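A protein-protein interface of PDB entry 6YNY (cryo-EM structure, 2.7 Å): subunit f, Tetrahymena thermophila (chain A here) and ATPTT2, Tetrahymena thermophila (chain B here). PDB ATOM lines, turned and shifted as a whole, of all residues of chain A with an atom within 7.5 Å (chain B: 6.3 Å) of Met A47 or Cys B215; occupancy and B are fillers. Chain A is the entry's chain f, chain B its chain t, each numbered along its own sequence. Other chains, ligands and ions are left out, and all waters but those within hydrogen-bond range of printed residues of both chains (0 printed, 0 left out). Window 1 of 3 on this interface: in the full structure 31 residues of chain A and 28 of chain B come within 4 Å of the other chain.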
ATOM      1  N   HIS A  29       9.519 -20.741  10.705  1.00  0.00           N
ATOM      2  CA  HIS A  29       9.651 -19.555   9.878  1.00  0.00           C
ATOM      3  C   HIS A  29      10.531 -19.793   8.663  1.00  0.00           C
ATOM      4  O   HIS A  29      10.668 -18.895   7.829  1.00  0.00           O
ATOM      5  CB  HIS A  29      10.219 -18.399  10.703  1.00  0.00           C
ATOM      6  CG  HIS A  29       9.443 -18.102  11.945  1.00  0.00           C
ATOM      7  ND1 HIS A  29       8.181 -17.549  11.920  1.00  0.00           N
ATOM      8  CD2 HIS A  29       9.754 -18.269  13.251  1.00  0.00           C
ATOM      9  CE1 HIS A  29       7.747 -17.394  13.157  1.00  0.00           C
ATOM     10  NE2 HIS A  29       8.682 -17.823  13.983  1.00  0.00           N
ATOM     11  N   GLY A  30      11.123 -20.977   8.542  1.00  0.00           N
ATOM     12  CA  GLY A  30      11.973 -21.310   7.422  1.00  0.00           C
ATOM     13  C   GLY A  30      13.457 -21.356   7.704  1.00  0.00           C
ATOM     14  O   GLY A  30      14.237 -21.531   6.763  1.00  0.00           O
ATOM     15  N   LYS A  41      17.850 -16.998  -3.295  1.00  0.00           N
ATOM     16  CA  LYS A  41      18.302 -17.267  -1.935  1.00  0.00           C
ATOM     17  C   LYS A  41      18.069 -16.073  -1.016  1.00  0.00           C
ATOM     18  O   LYS A  41      17.448 -16.203   0.044  1.00  0.00           O
ATOM     19  CB  LYS A  41      19.782 -17.642  -1.979  1.00  0.00           C
ATOM     20  CG  LYS A  41      20.485 -17.799  -0.658  1.00  0.00           C
ATOM     21  CD  LYS A  41      21.968 -17.690  -0.888  1.00  0.00           C
ATOM     22  CE  LYS A  41      22.771 -18.062   0.327  1.00  0.00           C
ATOM     23  NZ  LYS A  41      24.226 -18.063   0.015  1.00  0.00           N
ATOM     24  N   LYS A  42      18.567 -14.900  -1.406  1.00  0.00           N
ATOM     25  CA  LYS A  42      18.450 -13.731  -0.542  1.00  0.00           C
ATOM     26  C   LYS A  42      16.996 -13.342  -0.326  1.00  0.00           C
ATOM     27  O   LYS A  42      16.640 -12.843   0.747  1.00  0.00           O
ATOM     28  CB  LYS A  42      19.235 -12.563  -1.134  1.00  0.00           C
ATOM     29  CG  LYS A  42      20.715 -12.827  -1.282  1.00  0.00           C
ATOM     30  CD  LYS A  42      21.405 -11.706  -2.022  1.00  0.00           C
ATOM     31  CE  LYS A  42      22.880 -11.987  -2.208  1.00  0.00           C
ATOM     32  NZ  LYS A  42      23.124 -13.206  -3.037  1.00  0.00           N
ATOM     33  N   GLU A  43      16.143 -13.561  -1.326  1.00  0.00           N
ATOM     34  CA  GLU A  43      14.731 -13.240  -1.170  1.00  0.00           C
ATOM     35  C   GLU A  43      14.067 -14.153  -0.150  1.00  0.00           C
ATOM     36  O   GLU A  43      13.137 -13.732   0.545  1.00  0.00           O
ATOM     37  CB  GLU A  43      14.014 -13.336  -2.514  1.00  0.00           C
ATOM     38  CG  GLU A  43      14.437 -12.305  -3.539  1.00  0.00           C
ATOM     39  CD  GLU A  43      15.745 -12.640  -4.226  1.00  0.00           C
ATOM     40  OE1 GLU A  43      15.710 -13.004  -5.418  1.00  0.00           O
ATOM     41  OE2 GLU A  43      16.808 -12.547  -3.579  1.00  0.00           O
ATOM     42  N   ARG A  44      14.523 -15.401  -0.053  1.00  0.00           N
ATOM     43  CA  ARG A  44      13.964 -16.327   0.923  1.00  0.00           C
ATOM     44  C   ARG A  44      14.257 -15.863   2.343  1.00  0.00           C
ATOM     45  O   ARG A  44      13.371 -15.884   3.204  1.00  0.00           O
ATOM     46  CB  ARG A  44      14.527 -17.730   0.701  1.00  0.00           C
ATOM     47  CG  ARG A  44      14.454 -18.250  -0.728  1.00  0.00           C
ATOM     48  CD  ARG A  44      13.151 -18.907  -1.046  1.00  0.00           C
ATOM     49  NE  ARG A  44      12.969 -20.136  -0.288  1.00  0.00           N
ATOM     50  CZ  ARG A  44      12.024 -21.030  -0.544  1.00  0.00           C
ATOM     51  NH1 ARG A  44      11.929 -22.119   0.201  1.00  0.00           N
ATOM     52  NH2 ARG A  44      11.185 -20.841  -1.551  1.00  0.00           N
ATOM     53  N   TYR A  45      15.497 -15.443   2.605  1.00  0.00           N
ATOM     54  CA  TYR A  45      15.861 -14.983   3.941  1.00  0.00           C
ATOM     55  C   TYR A  45      15.001 -13.806   4.371  1.00  0.00           C
ATOM     56  O   TYR A  45      14.643 -13.687   5.548  1.00  0.00           O
ATOM     57  CB  TYR A  45      17.337 -14.596   3.979  1.00  0.00           C
ATOM     58  CG  TYR A  45      18.291 -15.753   4.159  1.00  0.00           C
ATOM     59  CD1 TYR A  45      18.613 -16.220   5.422  1.00  0.00           C
ATOM     60  CD2 TYR A  45      18.881 -16.368   3.070  1.00  0.00           C
ATOM     61  CE1 TYR A  45      19.484 -17.269   5.594  1.00  0.00           C
ATOM     62  CE2 TYR A  45      19.754 -17.419   3.232  1.00  0.00           C
ATOM     63  CZ  TYR A  45      20.054 -17.867   4.499  1.00  0.00           C
ATOM     64  OH  TYR A  45      20.925 -18.916   4.677  1.00  0.00           O
ATOM     65  N   GLU A  46      14.668 -12.922   3.434  1.00  0.00           N
ATOM     66  CA  GLU A  46      13.855 -11.762   3.769  1.00  0.00           C
ATOM     67  C   GLU A  46      12.480 -12.179   4.271  1.00  0.00           C
ATOM     68  O   GLU A  46      11.917 -11.540   5.166  1.00  0.00           O
ATOM     69  CB  GLU A  46      13.733 -10.854   2.549  1.00  0.00           C
ATOM     70  CG  GLU A  46      12.779  -9.695   2.728  1.00  0.00           C
ATOM     71  CD  GLU A  46      13.138  -8.819   3.906  1.00  0.00           C
ATOM     72  OE1 GLU A  46      14.308  -8.852   4.337  1.00  0.00           O
ATOM     73  OE2 GLU A  46      12.248  -8.099   4.405  1.00  0.00           O
ATOM     74  N   MET A  47      11.921 -13.245   3.703  1.00  0.00           N
ATOM     75  CA  MET A  47      10.613 -13.717   4.138  1.00  0.00           C
ATOM     76  C   MET A  47      10.692 -14.412   5.488  1.00  0.00           C
ATOM     77  O   MET A  47       9.720 -14.396   6.250  1.00  0.00           O
ATOM     78  CB  MET A  47      10.032 -14.652   3.086  1.00  0.00           C
ATOM     79  CG  MET A  47      10.014 -14.063   1.700  1.00  0.00           C
ATOM     80  SD  MET A  47       9.121 -12.512   1.590  1.00  0.00           S
ATOM     81  CE  MET A  47       7.474 -13.092   1.923  1.00  0.00           C
ATOM     82  N   ILE A  48      11.829 -15.035   5.795  1.00  0.00           N
ATOM     83  CA  ILE A  48      12.041 -15.579   7.131  1.00  0.00           C
ATOM     84  C   ILE A  48      12.118 -14.448   8.147  1.00  0.00           C
ATOM     85  O   ILE A  48      11.495 -14.501   9.214  1.00  0.00           O
ATOM     86  CB  ILE A  48      13.315 -16.441   7.160  1.00  0.00           C
ATOM     87  CG1 ILE A  48      13.247 -17.545   6.109  1.00  0.00           C
ATOM     88  CG2 ILE A  48      13.513 -17.044   8.534  1.00  0.00           C
ATOM     89  CD1 ILE A  48      14.564 -18.212   5.848  1.00  0.00           C
ATOM     90  N   TRP A  49      12.879 -13.402   7.825  1.00  0.00           N
ATOM     91  CA  TRP A  49      13.024 -12.269   8.729  1.00  0.00           C
ATOM     92  C   TRP A  49      11.692 -11.569   8.951  1.00  0.00           C
ATOM     93  O   TRP A  49      11.394 -11.118  10.061  1.00  0.00           O
ATOM     94  CB  TRP A  49      14.061 -11.303   8.159  1.00  0.00           C
ATOM     95  CG  TRP A  49      14.430 -10.175   9.050  1.00  0.00           C
ATOM     96  CD1 TRP A  49      14.125  -8.863   8.872  1.00  0.00           C
ATOM     97  CD2 TRP A  49      15.188 -10.251  10.258  1.00  0.00           C
ATOM     98  NE1 TRP A  49      14.643  -8.114   9.892  1.00  0.00           N
ATOM     99  CE2 TRP A  49      15.301  -8.944  10.760  1.00  0.00           C
ATOM    100  CE3 TRP A  49      15.780 -11.299  10.965  1.00  0.00           C
ATOM    101  CZ2 TRP A  49      15.980  -8.655  11.935  1.00  0.00           C
ATOM    102  CZ3 TRP A  49      16.453 -11.010  12.130  1.00  0.00           C
ATOM    103  CH2 TRP A  49      16.547  -9.701  12.604  1.00  0.00           C
ATOM    104  N   ARG A  50      10.876 -11.475   7.905  1.00  0.00           N
ATOM    105  CA  ARG A  50       9.580 -10.824   8.031  1.00  0.00           C
ATOM    106  C   ARG A  50       8.614 -11.677   8.842  1.00  0.00           C
ATOM    107  O   ARG A  50       7.793 -11.146   9.598  1.00  0.00           O
ATOM    108  CB  ARG A  50       9.024 -10.538   6.640  1.00  0.00           C
ATOM    109  CG  ARG A  50       7.722  -9.781   6.615  1.00  0.00           C
ATOM    110  CD  ARG A  50       7.199  -9.674   5.197  1.00  0.00           C
ATOM    111  NE  ARG A  50       8.209  -9.151   4.284  1.00  0.00           N
ATOM    112  CZ  ARG A  50       8.124  -9.224   2.963  1.00  0.00           C
ATOM    113  NH1 ARG A  50       7.080  -9.805   2.394  1.00  0.00           N
ATOM    114  NH2 ARG A  50       9.086  -8.726   2.207  1.00  0.00           N
ATOM    115  N   SER A  51       8.700 -12.999   8.702  1.00  0.00           N
ATOM    116  CA  SER A  51       7.838 -13.886   9.474  1.00  0.00           C
ATOM    117  C   SER A  51       8.214 -13.870  10.949  1.00  0.00           C
ATOM    118  O   SER A  51       7.337 -13.896  11.819  1.00  0.00           O
ATOM    119  CB  SER A  51       7.922 -15.305   8.916  1.00  0.00           C
ATOM    120  OG  SER A  51       6.964 -16.154   9.511  1.00  0.00           O
ATOM    121  N   MET A  52       9.511 -13.834  11.249  1.00  0.00           N
ATOM    122  CA  MET A  52       9.948 -13.751  12.636  1.00  0.00           C
ATOM    123  C   MET A  52       9.538 -12.433  13.279  1.00  0.00           C
ATOM    124  O   MET A  52       9.299 -12.386  14.489  1.00  0.00           O
ATOM    125  CB  MET A  52      11.464 -13.923  12.712  1.00  0.00           C
ATOM    126  CG  MET A  52      11.963 -15.270  12.229  1.00  0.00           C
ATOM    127  SD  MET A  52      13.707 -15.282  11.794  1.00  0.00           S
ATOM    128  CE  MET A  52      14.444 -14.886  13.368  1.00  0.00           C
ATOM    129  N   GLY A  53       9.449 -11.363  12.497  1.00  0.00           N
ATOM    130  CA  GLY A  53       9.105 -10.065  13.038  1.00  0.00           C
ATOM    131  C   GLY A  53       7.635  -9.901  13.351  1.00  0.00           C
ATOM    132  O   GLY A  53       7.277  -9.295  14.364  1.00  0.00           O
ATOM    133  N   LYS A  54       6.771 -10.431  12.486  1.00  0.00           N
ATOM    134  CA  LYS A  54       5.338 -10.369  12.748  1.00  0.00           C
ATOM    135  C   LYS A  54       4.972 -11.121  14.016  1.00  0.00           C
ATOM    136  O   LYS A  54       4.025 -10.742  14.714  1.00  0.00           O
ATOM    137  CB  LYS A  54       4.564 -10.934  11.562  1.00  0.00           C
ATOM    138  CG  LYS A  54       4.604 -10.066  10.324  1.00  0.00           C
ATOM    139  CD  LYS A  54       4.068 -10.806   9.107  1.00  0.00           C
ATOM    140  CE  LYS A  54       2.626 -11.258   9.300  1.00  0.00           C
ATOM    141  NZ  LYS A  54       1.704 -10.124   9.606  1.00  0.00           N
ATOM    142  N   ALA B 210       1.250  -3.953  -7.551  1.00  0.00           N
ATOM    143  CA  ALA B 210       0.308  -5.006  -7.197  1.00  0.00           C
ATOM    144  C   ALA B 210       1.031  -6.216  -6.625  1.00  0.00           C
ATOM    145  O   ALA B 210       0.616  -6.780  -5.607  1.00  0.00           O
ATOM    146  CB  ALA B 210      -0.510  -5.399  -8.421  1.00  0.00           C
ATOM    147  N   LEU B 211       2.114  -6.634  -7.276  1.00  0.00           N
ATOM    148  CA  LEU B 211       2.849  -7.801  -6.813  1.00  0.00           C
ATOM    149  C   LEU B 211       3.531  -7.537  -5.481  1.00  0.00           C
ATOM    150  O   LEU B 211       3.682  -8.457  -4.670  1.00  0.00           O
ATOM    151  CB  LEU B 211       3.874  -8.207  -7.866  1.00  0.00           C
ATOM    152  CG  LEU B 211       4.665  -9.483  -7.627  1.00  0.00           C
ATOM    153  CD1 LEU B 211       3.762 -10.689  -7.568  1.00  0.00           C
ATOM    154  CD2 LEU B 211       5.664  -9.636  -8.732  1.00  0.00           C
ATOM    155  N   ALA B 212       3.954  -6.295  -5.243  1.00  0.00           N
ATOM    156  CA  ALA B 212       4.587  -5.956  -3.976  1.00  0.00           C
ATOM    157  C   ALA B 212       3.625  -6.150  -2.816  1.00  0.00           C
ATOM    158  O   ALA B 212       4.023  -6.590  -1.733  1.00  0.00           O
ATOM    159  CB  ALA B 212       5.093  -4.518  -4.017  1.00  0.00           C
ATOM    160  N   VAL B 213       2.351  -5.823  -3.025  1.00  0.00           N
ATOM    161  CA  VAL B 213       1.360  -5.987  -1.968  1.00  0.00           C
ATOM    162  C   VAL B 213       1.222  -7.457  -1.599  1.00  0.00           C
ATOM    163  O   VAL B 213       1.135  -7.810  -0.417  1.00  0.00           O
ATOM    164  CB  VAL B 213       0.014  -5.385  -2.409  1.00  0.00           C
ATOM    165  CG1 VAL B 213      -1.027  -5.551  -1.323  1.00  0.00           C
ATOM    166  CG2 VAL B 213       0.171  -3.927  -2.763  1.00  0.00           C
ATOM    167  N   GLY B 214       1.193  -8.334  -2.600  1.00  0.00           N
ATOM    168  CA  GLY B 214       1.173  -9.756  -2.320  1.00  0.00           C
ATOM    169  C   GLY B 214       2.433 -10.239  -1.636  1.00  0.00           C
ATOM    170  O   GLY B 214       2.402 -11.217  -0.886  1.00  0.00           O
ATOM    171  N   CYS B 215       3.557  -9.566  -1.883  1.00  0.00           N
ATOM    172  CA  CYS B 215       4.802  -9.951  -1.233  1.00  0.00           C
ATOM    173  C   CYS B 215       4.816  -9.531   0.229  1.00  0.00           C
ATOM    174  O   CYS B 215       5.320 -10.267   1.086  1.00  0.00           O
ATOM    175  CB  CYS B 215       5.984  -9.346  -1.980  1.00  0.00           C
ATOM    176  SG  CYS B 215       6.167  -9.953  -3.665  1.00  0.00           S
ATOM    177  N   TYR B 216       4.273  -8.357   0.536  1.00  0.00           N
ATOM    178  CA  TYR B 216       4.254  -7.875   1.910  1.00  0.00           C
ATOM    179  C   TYR B 216       2.994  -8.271   2.660  1.00  0.00           C
ATOM    180  O   TYR B 216       3.046  -8.457   3.881  1.00  0.00           O
ATOM    181  CB  TYR B 216       4.406  -6.355   1.936  1.00  0.00           C
ATOM    182  CG  TYR B 216       5.785  -5.878   1.573  1.00  0.00           C
ATOM    183  CD1 TYR B 216       6.807  -5.887   2.505  1.00  0.00           C
ATOM    184  CD2 TYR B 216       6.066  -5.411   0.304  1.00  0.00           C
ATOM    185  CE1 TYR B 216       8.064  -5.453   2.181  1.00  0.00           C
ATOM    186  CE2 TYR B 216       7.323  -4.975  -0.029  1.00  0.00           C
ATOM    187  CZ  TYR B 216       8.318  -4.997   0.913  1.00  0.00           C
ATOM    188  OH  TYR B 216       9.576  -4.559   0.580  1.00  0.00           O
ATOM    189  N   HIS B 217       1.862  -8.395   1.971  1.00  0.00           N
ATOM    190  CA  HIS B 217       0.602  -8.809   2.585  1.00  0.00           C
ATOM    191  C   HIS B 217      -0.010  -9.895   1.711  1.00  0.00           C
ATOM    192  O   HIS B 217      -0.838  -9.613   0.843  1.00  0.00           O
ATOM    193  CB  HIS B 217      -0.333  -7.625   2.760  1.00  0.00           C
ATOM    194  CG  HIS B 217       0.258  -6.514   3.567  1.00  0.00           C
ATOM    195  ND1 HIS B 217       0.996  -5.499   3.003  1.00  0.00           N
ATOM    196  CD2 HIS B 217       0.237  -6.270   4.898  1.00  0.00           C
ATOM    197  CE1 HIS B 217       1.397  -4.672   3.950  1.00  0.00           C
ATOM    198  NE2 HIS B 217       0.949  -5.115   5.109  1.00  0.00           N
ATOM    199  N   ALA B 218       0.387 -11.138   1.957  1.00  0.00           N
ATOM    200  CA  ALA B 218      -0.077 -12.261   1.155  1.00  0.00           C
ATOM    201  C   ALA B 218      -1.326 -12.903   1.730  1.00  0.00           C
ATOM    202  O   ALA B 218      -2.158 -13.412   0.971  1.00  0.00           O
ATOM    203  CB  ALA B 218       1.026 -13.310   1.037  1.00  0.00           C
ATOM    204  N   TRP B 317      13.560  -3.135  -8.829  1.00  0.00           N
ATOM    205  CA  TRP B 317      12.917  -4.133  -7.982  1.00  0.00           C
ATOM    206  C   TRP B 317      13.962  -4.656  -7.007  1.00  0.00           C
ATOM    207  O   TRP B 317      14.924  -5.315  -7.414  1.00  0.00           O
ATOM    208  CB  TRP B 317      12.325  -5.275  -8.801  1.00  0.00           C
ATOM    209  CG  TRP B 317      11.703  -6.317  -7.941  1.00  0.00           C
ATOM    210  CD1 TRP B 317      12.330  -7.375  -7.366  1.00  0.00           C
ATOM    211  CD2 TRP B 317      10.333  -6.398  -7.543  1.00  0.00           C
ATOM    212  NE1 TRP B 317      11.439  -8.113  -6.633  1.00  0.00           N
ATOM    213  CE2 TRP B 317      10.204  -7.534  -6.728  1.00  0.00           C
ATOM    214  CE3 TRP B 317       9.203  -5.624  -7.799  1.00  0.00           C
ATOM    215  CZ2 TRP B 317       8.994  -7.911  -6.168  1.00  0.00           C
ATOM    216  CZ3 TRP B 317       8.006  -6.001  -7.243  1.00  0.00           C
ATOM    217  CH2 TRP B 317       7.909  -7.132  -6.438  1.00  0.00           C
ATOM    218  N   LYS B 320      14.726  -6.717  -1.219  1.00  0.00           N
ATOM    219  CA  LYS B 320      13.978  -6.522   0.017  1.00  0.00           C
ATOM    220  C   LYS B 320      12.509  -6.882  -0.135  1.00  0.00           C
ATOM    221  O   LYS B 320      11.855  -7.236   0.851  1.00  0.00           O
ATOM    222  CB  LYS B 320      14.106  -5.068   0.458  1.00  0.00           C
ATOM    223  CG  LYS B 320      13.323  -4.718   1.696  1.00  0.00           C
ATOM    224  CD  LYS B 320      13.452  -3.250   2.015  1.00  0.00           C
ATOM    225  CE  LYS B 320      12.676  -2.407   1.039  1.00  0.00           C
ATOM    226  NZ  LYS B 320      12.664  -0.984   1.444  1.00  0.00           N
ATOM    227  N   ASN B 321      11.966  -6.791  -1.348  1.00  0.00           N
ATOM    228  CA  ASN B 321      10.540  -7.032  -1.517  1.00  0.00           C
ATOM    229  C   ASN B 321      10.186  -8.488  -1.260  1.00  0.00           C
ATOM    230  O   ASN B 321       9.044  -8.794  -0.904  1.00  0.00           O
ATOM    231  CB  ASN B 321      10.102  -6.599  -2.912  1.00  0.00           C
ATOM    232  CG  ASN B 321      10.283  -5.118  -3.139  1.00  0.00           C
ATOM    233  OD1 ASN B 321      10.216  -4.323  -2.203  1.00  0.00           O
ATOM    234  ND2 ASN B 321      10.515  -4.736  -4.382  1.00  0.00           N
ATOM    235  N   GLY B 322      11.141  -9.392  -1.438  1.00  0.00           N
ATOM    236  CA  GLY B 322      10.952 -10.771  -1.055  1.00  0.00           C
ATOM    237  C   GLY B 322      10.326 -11.637  -2.123  1.00  0.00           C
ATOM    238  O   GLY B 322      10.646 -11.521  -3.309  1.00  0.00           O
ATOM    239  N   ILE B 323       9.429 -12.518  -1.696  1.00  0.00           N
ATOM    240  CA  ILE B 323       8.805 -13.503  -2.565  1.00  0.00           C
ATOM    241  C   ILE B 323       7.299 -13.415  -2.400  1.00  0.00           C
ATOM    242  O   ILE B 323       6.800 -13.153  -1.301  1.00  0.00           O
ATOM    243  CB  ILE B 323       9.309 -14.926  -2.242  1.00  0.00           C
ATOM    244  CG1 ILE B 323      10.751 -15.081  -2.719  1.00  0.00           C
ATOM    245  CG2 ILE B 323       8.397 -15.978  -2.845  1.00  0.00           C
ATOM    246  CD1 ILE B 323      11.360 -16.390  -2.392  1.00  0.00           C
ATOM    247  N   TYR B 324       6.578 -13.631  -3.492  1.00  0.00           N
ATOM    248  CA  TYR B 324       5.129 -13.717  -3.465  1.00  0.00           C
ATOM    249  C   TYR B 324       4.737 -15.185  -3.417  1.00  0.00           C
ATOM    250  O   TYR B 324       5.180 -15.977  -4.254  1.00  0.00           O
ATOM    251  CB  TYR B 324       4.504 -13.034  -4.677  1.00  0.00           C
ATOM    252  CG  TYR B 324       3.011 -13.210  -4.758  1.00  0.00           C
ATOM    253  CD1 TYR B 324       2.200 -12.920  -3.673  1.00  0.00           C
ATOM    254  CD2 TYR B 324       2.412 -13.666  -5.913  1.00  0.00           C
ATOM    255  CE1 TYR B 324       0.841 -13.083  -3.741  1.00  0.00           C
ATOM    256  CE2 TYR B 324       1.055 -13.828  -5.990  1.00  0.00           C
ATOM    257  CZ  TYR B 324       0.272 -13.535  -4.902  1.00  0.00           C
ATOM    258  OH  TYR B 324      -1.087 -13.699  -4.975  1.00  0.00           O
ATOM    259  N   THR B 325       3.915 -15.541  -2.440  1.00  0.00           N
ATOM    260  CA  THR B 325       3.599 -16.932  -2.166  1.00  0.00           C
ATOM    261  C   THR B 325       2.361 -17.427  -2.898  1.00  0.00           C
ATOM    262  O   THR B 325       2.129 -18.639  -2.938  1.00  0.00           O
ATOM    263  CB  THR B 325       3.406 -17.133  -0.664  1.00  0.00           C
ATOM    264  OG1 THR B 325       2.617 -16.064  -0.131  1.00  0.00           O
ATOM    265  CG2 THR B 325       4.737 -17.170   0.043  1.00  0.00           C
ATOM    266  N   VAL B 351      10.840 -14.479  -8.187  1.00  0.00           N
ATOM    267  CA  VAL B 351      10.076 -13.766  -7.181  1.00  0.00           C
ATOM    268  C   VAL B 351       8.779 -14.473  -6.813  1.00  0.00           C
ATOM    269  O   VAL B 351       8.328 -14.350  -5.669  1.00  0.00           O
ATOM    270  CB  VAL B 351       9.793 -12.327  -7.653  1.00  0.00           C
ATOM    271  CG1 VAL B 351       8.782 -11.660  -6.756  1.00  0.00           C
ATOM    272  CG2 VAL B 351      11.074 -11.532  -7.687  1.00  0.00           C
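Printed residues of chain B within 4 Å of Arg A44: Ile B323. Printed residues of chain B within 4 Å of Glu A46: Lys B320 (3.2 Å). Met A47 touches just these residues of chain B: Cys B215 (3.6 Å), Gly B322 (3.7 Å) and Ile B323 (3.3 Å). Printed residues of chain B within 4 Å of Arg A50: Cys B215, Tyr B216, Lys B320 and Asn B321. Gly B214 touches none of the printed residues of chain A. Cys B215 touches just these residues of chain A: Met A47 (3.6 Å) and Arg A50 (2.2 Å). Ala B218 touches none of the printed residues of chain A. Printed residues of chain A within 4 Å of Ile B323: Glu A43 (3.7 Å), Arg A44 (3.4 Å) and Met A47 (3.3 Å). The nearest residue of chain B that does not touch Met A47 is Asn B321 (4.5 Å). The nearest printed residue of chain A that does not touch Cys B215 is Glu A46 (7.7 Å).
Glu A43 touches Gly B322 (CG to O, 3.9 Å). Glu A43 touches Ile B323. Ile B323 touches Arg A44 (CD1 to CD, 3.4 Å). Glu A46 touches Lys B320 (CG to O, 3.2 Å). CE of Met A47 touches O of Cys B215, 3.6 Å away. Met A47 touches Gly B322 (SD to CA, 3.7 Å). NH2 of Arg A50 touches CE1 of Tyr B216, 3.4 Å away.
NH2 of Arg A50 is in hydrogen-bond range of O of Lys B320, at 3.4 Å. NH2 of Arg A50 sits at hydrogen-bond distance from O of Asn B321, 3.1 Å away. The side-chain sulfur (SD) of Met A47 lies within hydrogen-bond range of the backbone NH (N) of Ile B323 (3.3 Å). NH1 of Arg A50 lies close to O of Cys B215, at 2.2 Å.
Hydrophobic or aromatic side chains of chain B within 4 Å of the printed part of chain A: Tyr B216 and Ile B323. Along chain B the printed residues that touch a printed residue of chain A span positions 215 to 323. Hydrophobic or aromatic side chains of chain A that line the printed part of chain B: Met A47. Along chain A the printed residues that touch a printed residue of chain B span positions 43 to 50. Among the printed residues, no Asp or Glu carboxylate lies within 4 Å of a Lys or Arg side-chain nitrogen of the other chain.
O of Leu B211 is in hydrogen-bond range of SG of Cys B215 (3.1 Å). N of Tyr B324 lies close to SG of Cys B215, 3.7 Å away. The side-chain amide oxygen (OD1) of Asn B321 is in hydrogen-bond range of the side-chain hydroxyl (OH) of Tyr B216. The guanidinium group (NH2) of Arg A50 lies within salt-bridge range of the side-chain carboxylate (OE2) of Glu A46 (3.9 Å). The guanidinium group (NH1) of Arg A50 lies close to the side-chain sulfur (SD) of Met A47 (3.5 Å).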
